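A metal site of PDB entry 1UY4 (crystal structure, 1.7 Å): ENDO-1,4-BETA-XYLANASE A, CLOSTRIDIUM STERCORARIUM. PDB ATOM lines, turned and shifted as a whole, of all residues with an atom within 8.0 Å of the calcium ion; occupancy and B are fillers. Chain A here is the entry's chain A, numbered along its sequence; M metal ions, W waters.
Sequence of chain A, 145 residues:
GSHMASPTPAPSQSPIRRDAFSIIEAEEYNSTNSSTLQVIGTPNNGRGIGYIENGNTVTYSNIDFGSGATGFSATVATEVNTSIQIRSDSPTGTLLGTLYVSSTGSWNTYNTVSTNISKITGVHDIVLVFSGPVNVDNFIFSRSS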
ATOM      1  N   ILE A  23      16.054  11.375  -8.592  1.00  0.00           N
ATOM      2  CA  ILE A  23      15.894  12.023  -7.318  1.00  0.00           C
ATOM      3  C   ILE A  23      17.209  12.030  -6.585  1.00  0.00           C
ATOM      4  O   ILE A  23      17.903  11.003  -6.470  1.00  0.00           O
ATOM      5  CB  ILE A  23      14.807  11.331  -6.476  1.00  0.00           C
ATOM      6  CG1 ILE A  23      13.419  11.591  -7.117  1.00  0.00           C
ATOM      7  CG2 ILE A  23      14.857  11.760  -4.992  1.00  0.00           C
ATOM      8  CD1 ILE A  23      12.867  12.929  -6.948  1.00  0.00           C
ATOM      9  N   ILE A  24      17.531  13.201  -6.080  1.00  0.00           N
ATOM     10  CA  ILE A  24      18.682  13.394  -5.183  1.00  0.00           C
ATOM     11  C   ILE A  24      18.135  13.720  -3.797  1.00  0.00           C
ATOM     12  O   ILE A  24      17.307  14.627  -3.622  1.00  0.00           O
ATOM     13  CB  ILE A  24      19.616  14.549  -5.727  1.00  0.00           C
ATOM     14  CG1 ILE A  24      20.163  14.190  -7.129  1.00  0.00           C
ATOM     15  CG2 ILE A  24      20.741  14.862  -4.707  1.00  0.00           C
ATOM     16  CD1 ILE A  24      20.696  15.425  -7.889  1.00  0.00           C
ATOM     17  N   GLU A  25      18.551  12.946  -2.792  1.00  0.00           N
ATOM     18  CA  GLU A  25      18.059  13.106  -1.432  1.00  0.00           C
ATOM     19  C   GLU A  25      18.861  14.226  -0.755  1.00  0.00           C
ATOM     20  O   GLU A  25      20.087  14.177  -0.705  1.00  0.00           O
ATOM     21  CB  GLU A  25      18.137  11.806  -0.634  1.00  0.00           C
ATOM     22  CG  GLU A  25      17.280  10.720  -1.216  1.00  0.00           C
ATOM     23  CD  GLU A  25      15.802  10.988  -1.087  1.00  0.00           C
ATOM     24  OE1 GLU A  25      15.407  11.983  -0.427  1.00  0.00           O
ATOM     25  OE2 GLU A  25      15.039  10.171  -1.603  1.00  0.00           O
ATOM     26  N   ALA A  26      18.152  15.230  -0.265  1.00  0.00           N
ATOM     27  CA  ALA A  26      18.805  16.398   0.315  1.00  0.00           C
ATOM     28  C   ALA A  26      19.688  16.028   1.533  1.00  0.00           C
ATOM     29  O   ALA A  26      20.716  16.674   1.783  1.00  0.00           O
ATOM     30  CB  ALA A  26      17.801  17.484   0.655  1.00  0.00           C
ATOM     31  N   GLU A  27      19.285  15.018   2.300  1.00  0.00           N
ATOM     32  CA  GLU A  27      19.997  14.559   3.488  1.00  0.00           C
ATOM     33  C   GLU A  27      21.298  13.838   3.141  1.00  0.00           C
ATOM     34  O   GLU A  27      22.126  13.626   4.013  1.00  0.00           O
ATOM     35  CB  GLU A  27      19.079  13.656   4.354  1.00  0.00           C
ATOM     36  CG  GLU A  27      18.624  12.345   3.678  1.00  0.00           C
ATOM     37  CD  GLU A  27      17.340  12.486   2.862  1.00  0.00           C
ATOM     38  OE1 GLU A  27      17.000  13.625   2.404  1.00  0.00           O
ATOM     39  OE2 GLU A  27      16.640  11.464   2.675  1.00  0.00           O
ATOM     40  N   GLU A  28      21.482  13.450   1.882  1.00  0.00           N
ATOM     41  CA  GLU A  28      22.694  12.814   1.420  1.00  0.00           C
ATOM     42  C   GLU A  28      23.671  13.836   0.788  1.00  0.00           C
ATOM     43  O   GLU A  28      24.155  13.648  -0.301  1.00  0.00           O
ATOM     44  CB  GLU A  28      22.389  11.657   0.461  1.00  0.00           C
ATOM     45  CG  GLU A  28      21.567  10.559   1.161  1.00  0.00           C
ATOM     46  CD  GLU A  28      21.165   9.422   0.258  1.00  0.00           C
ATOM     47  OE1 GLU A  28      20.471   8.524   0.749  1.00  0.00           O
ATOM     48  OE2 GLU A  28      21.512   9.399  -0.925  1.00  0.00           O
ATOM     49  N   VAL A  39      19.755  16.388   9.952  1.00  0.00           N
ATOM     50  CA  VAL A  39      18.936  15.448   9.193  1.00  0.00           C
ATOM     51  C   VAL A  39      17.663  15.278   9.995  1.00  0.00           C
ATOM     52  O   VAL A  39      17.725  14.994  11.211  1.00  0.00           O
ATOM     53  CB  VAL A  39      19.649  14.131   8.912  1.00  0.00           C
ATOM     54  CG1 VAL A  39      18.689  13.070   8.273  1.00  0.00           C
ATOM     55  CG2 VAL A  39      20.805  14.378   7.979  1.00  0.00           C
ATOM     56  N   ILE A  40      16.530  15.522   9.341  1.00  0.00           N
ATOM     57  CA  ILE A  40      15.222  15.467   9.964  1.00  0.00           C
ATOM     58  C   ILE A  40      14.392  14.344   9.329  1.00  0.00           C
ATOM     59  O   ILE A  40      14.712  13.830   8.262  1.00  0.00           O
ATOM     60  CB  ILE A  40      14.485  16.804   9.813  1.00  0.00           C
ATOM     61  CG1 ILE A  40      14.365  17.225   8.324  1.00  0.00           C
ATOM     62  CG2 ILE A  40      15.186  17.928  10.652  1.00  0.00           C
ATOM     63  CD1 ILE A  40      13.298  18.208   8.078  1.00  0.00           C
ATOM     64  N   THR A  42      10.458  13.165   7.941  1.00  0.00           N
ATOM     65  CA  THR A  42       9.287  13.741   7.275  1.00  0.00           C
ATOM     66  C   THR A  42       8.063  12.899   7.660  1.00  0.00           C
ATOM     67  O   THR A  42       8.210  11.815   8.186  1.00  0.00           O
ATOM     68  CB  THR A  42       9.449  13.711   5.713  1.00  0.00           C
ATOM     69  OG1 THR A  42       9.527  12.344   5.266  1.00  0.00           O
ATOM     70  CG2 THR A  42      10.724  14.417   5.269  1.00  0.00           C
ATOM     71  N   GLY A  46      10.222   9.497   5.558  1.00  0.00           N
ATOM     72  CA  GLY A  46      11.387   9.858   4.763  1.00  0.00           C
ATOM     73  C   GLY A  46      12.316  10.703   5.637  1.00  0.00           C
ATOM     74  O   GLY A  46      12.131  10.830   6.851  1.00  0.00           O
ATOM     75  N   ARG A  47      13.353  11.229   5.017  1.00  0.00           N
ATOM     76  CA  ARG A  47      14.270  12.188   5.659  1.00  0.00           C
ATOM     77  C   ARG A  47      14.494  13.426   4.794  1.00  0.00           C
ATOM     78  O   ARG A  47      14.139  13.465   3.633  1.00  0.00           O
ATOM     79  CB  ARG A  47      15.588  11.492   5.993  1.00  0.00           C
ATOM     80  CG  ARG A  47      15.414  10.240   6.942  1.00  0.00           C
ATOM     81  CD  ARG A  47      16.690   9.610   7.491  1.00  0.00           C
ATOM     82  NE  ARG A  47      16.750   9.940   8.929  1.00  0.00           N
ATOM     83  CZ  ARG A  47      17.859   9.995   9.730  1.00  0.00           C
ATOM     84  NH1 ARG A  47      19.072   9.691   9.267  1.00  0.00           N
ATOM     85  NH2 ARG A  47      17.720  10.360  11.029  1.00  0.00           N
ATOM     86  N   GLY A  48      15.078  14.440   5.413  1.00  0.00           N
ATOM     87  CA  GLY A  48      15.367  15.708   4.804  1.00  0.00           C
ATOM     88  C   GLY A  48      16.418  16.436   5.592  1.00  0.00           C
ATOM     89  O   GLY A  48      17.064  15.856   6.484  1.00  0.00           O
ATOM     90  N   ILE A  49      16.660  17.688   5.221  1.00  0.00           N
ATOM     91  CA  ILE A  49      17.509  18.558   6.008  1.00  0.00           C
ATOM     92  C   ILE A  49      16.660  19.691   6.498  1.00  0.00           C
ATOM     93  O   ILE A  49      15.741  20.151   5.808  1.00  0.00           O
ATOM     94  CB  ILE A  49      18.754  19.053   5.165  1.00  0.00           C
ATOM     95  CG1 ILE A  49      18.321  19.750   3.874  1.00  0.00           C
ATOM     96  CG2 ILE A  49      19.653  17.898   4.886  1.00  0.00           C
ATOM     97  CD1 ILE A  49      19.469  20.351   2.998  1.00  0.00           C
ATOM     98  N   THR A  75      11.460  19.434  -3.306  1.00  0.00           N
ATOM     99  CA  THR A  75      10.330  19.195  -2.431  1.00  0.00           C
ATOM    100  C   THR A  75      10.677  19.735  -1.051  1.00  0.00           C
ATOM    101  O   THR A  75      11.609  19.263  -0.398  1.00  0.00           O
ATOM    102  CB  THR A  75      10.023  17.678  -2.401  1.00  0.00           C
ATOM    103  OG1 THR A  75       9.662  17.228  -3.756  1.00  0.00           O
ATOM    104  CG2 THR A  75       8.825  17.384  -1.523  1.00  0.00           C
ATOM    105  N   TYR A 110       4.981  19.606   2.778  1.00  0.00           N
ATOM    106  CA  TYR A 110       5.916  19.668   1.629  1.00  0.00           C
ATOM    107  C   TYR A 110       5.203  19.966   0.311  1.00  0.00           C
ATOM    108  O   TYR A 110       4.070  19.538   0.100  1.00  0.00           O
ATOM    109  CB  TYR A 110       6.718  18.362   1.561  1.00  0.00           C
ATOM    110  CG  TYR A 110       7.754  18.270   2.675  1.00  0.00           C
ATOM    111  CD1 TYR A 110       7.404  17.814   3.901  1.00  0.00           C
ATOM    112  CD2 TYR A 110       9.064  18.730   2.480  1.00  0.00           C
ATOM    113  CE1 TYR A 110       8.315  17.761   4.967  1.00  0.00           C
ATOM    114  CE2 TYR A 110      10.013  18.678   3.507  1.00  0.00           C
ATOM    115  CZ  TYR A 110       9.633  18.220   4.775  1.00  0.00           C
ATOM    116  OH  TYR A 110      10.525  18.170   5.808  1.00  0.00           O
ATOM    117  N   VAL A 136      14.112  20.617   3.388  1.00  0.00           N
ATOM    118  CA  VAL A 136      14.264  20.057   2.045  1.00  0.00           C
ATOM    119  C   VAL A 136      14.314  18.564   2.130  1.00  0.00           C
ATOM    120  O   VAL A 136      15.205  17.991   2.809  1.00  0.00           O
ATOM    121  CB  VAL A 136      15.538  20.565   1.324  1.00  0.00           C
ATOM    122  CG1 VAL A 136      15.492  20.223  -0.152  1.00  0.00           C
ATOM    123  CG2 VAL A 136      15.730  22.103   1.526  1.00  0.00           C
ATOM    124  N   ASP A 137      13.394  17.910   1.406  1.00  0.00           N
ATOM    125  CA  ASP A 137      13.368  16.463   1.354  1.00  0.00           C
ATOM    126  C   ASP A 137      14.299  15.924   0.214  1.00  0.00           C
ATOM    127  O   ASP A 137      15.220  15.093   0.431  1.00  0.00           O
ATOM    128  CB  ASP A 137      11.880  15.999   1.183  1.00  0.00           C
ATOM    129  CG  ASP A 137      11.706  14.533   1.185  1.00  0.00           C
ATOM    130  OD1 ASP A 137      12.684  13.791   0.890  1.00  0.00           O
ATOM    131  OD2 ASP A 137      10.592  14.024   1.443  1.00  0.00           O
ATOM    132  N   ASN A 138      14.064  16.430  -0.985  1.00  0.00           N
ATOM    133  CA  ASN A 138      14.778  15.980  -2.195  1.00  0.00           C
ATOM    134  C   ASN A 138      14.720  17.041  -3.287  1.00  0.00           C
ATOM    135  O   ASN A 138      14.089  18.090  -3.094  1.00  0.00           O
ATOM    136  CB  ASN A 138      14.235  14.608  -2.664  1.00  0.00           C
ATOM    137  CG  ASN A 138      12.777  14.673  -3.180  1.00  0.00           C
ATOM    138  OD1 ASN A 138      11.993  13.694  -3.066  1.00  0.00           O
ATOM    139  ND2 ASN A 138      12.457  15.746  -3.798  1.00  0.00           N
ATOM    140  N   PHE A 139      15.407  16.784  -4.395  1.00  0.00           N
ATOM    141  CA  PHE A 139      15.391  17.621  -5.590  1.00  0.00           C
ATOM    142  C   PHE A 139      15.812  16.815  -6.798  1.00  0.00           C
ATOM    143  O   PHE A 139      16.324  15.739  -6.693  1.00  0.00           O
ATOM    144  CB  PHE A 139      16.221  18.913  -5.425  1.00  0.00           C
ATOM    145  CG  PHE A 139      17.650  18.684  -4.997  1.00  0.00           C
ATOM    146  CD1 PHE A 139      18.003  18.739  -3.628  1.00  0.00           C
ATOM    147  CD2 PHE A 139      18.626  18.498  -5.919  1.00  0.00           C
ATOM    148  CE1 PHE A 139      19.309  18.576  -3.217  1.00  0.00           C
ATOM    149  CE2 PHE A 139      19.960  18.311  -5.508  1.00  0.00           C
ATOM    150  CZ  PHE A 139      20.283  18.376  -4.167  1.00  0.00           C
HETATM  151 CA    CA M   1      14.793  12.945   1.501  1.00  0.00          CA
HETATM  152  O   HOH W   1      13.570  10.954   2.021  1.00  0.00           O
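O of Thr 75 is in hydrogen-bond range of N of Asp 137. The backbone NH of Ala 26 sits close to the backbone carbonyl oxygen of Asp 137 (3.0 Å).
Within 4 Å of the calcium ion: Glu 25, Glu 27, Arg 47 and Asp 137. Along chain A the residues within 4 Å of the calcium ion span positions 25 to 137.
OE1 of Glu 25 is bound to the calcium ion, 2.2 Å away. The backbone carbonyl oxygen (O) of Arg 47 is bound to the calcium ion (2.3 Å). The calcium ion is bound by the side-chain carboxylate (OD1) of Asp 137 (2.4 Å). The calcium ion is bound by water W1 (2.4 Å). The backbone carbonyl oxygen (O) of Asp 137 is bound to the calcium ion, at 2.4 Å. The calcium ion is bound by OE1 of Glu 27 (2.5 Å). The calcium ion is bound by OE2 of Glu 27.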
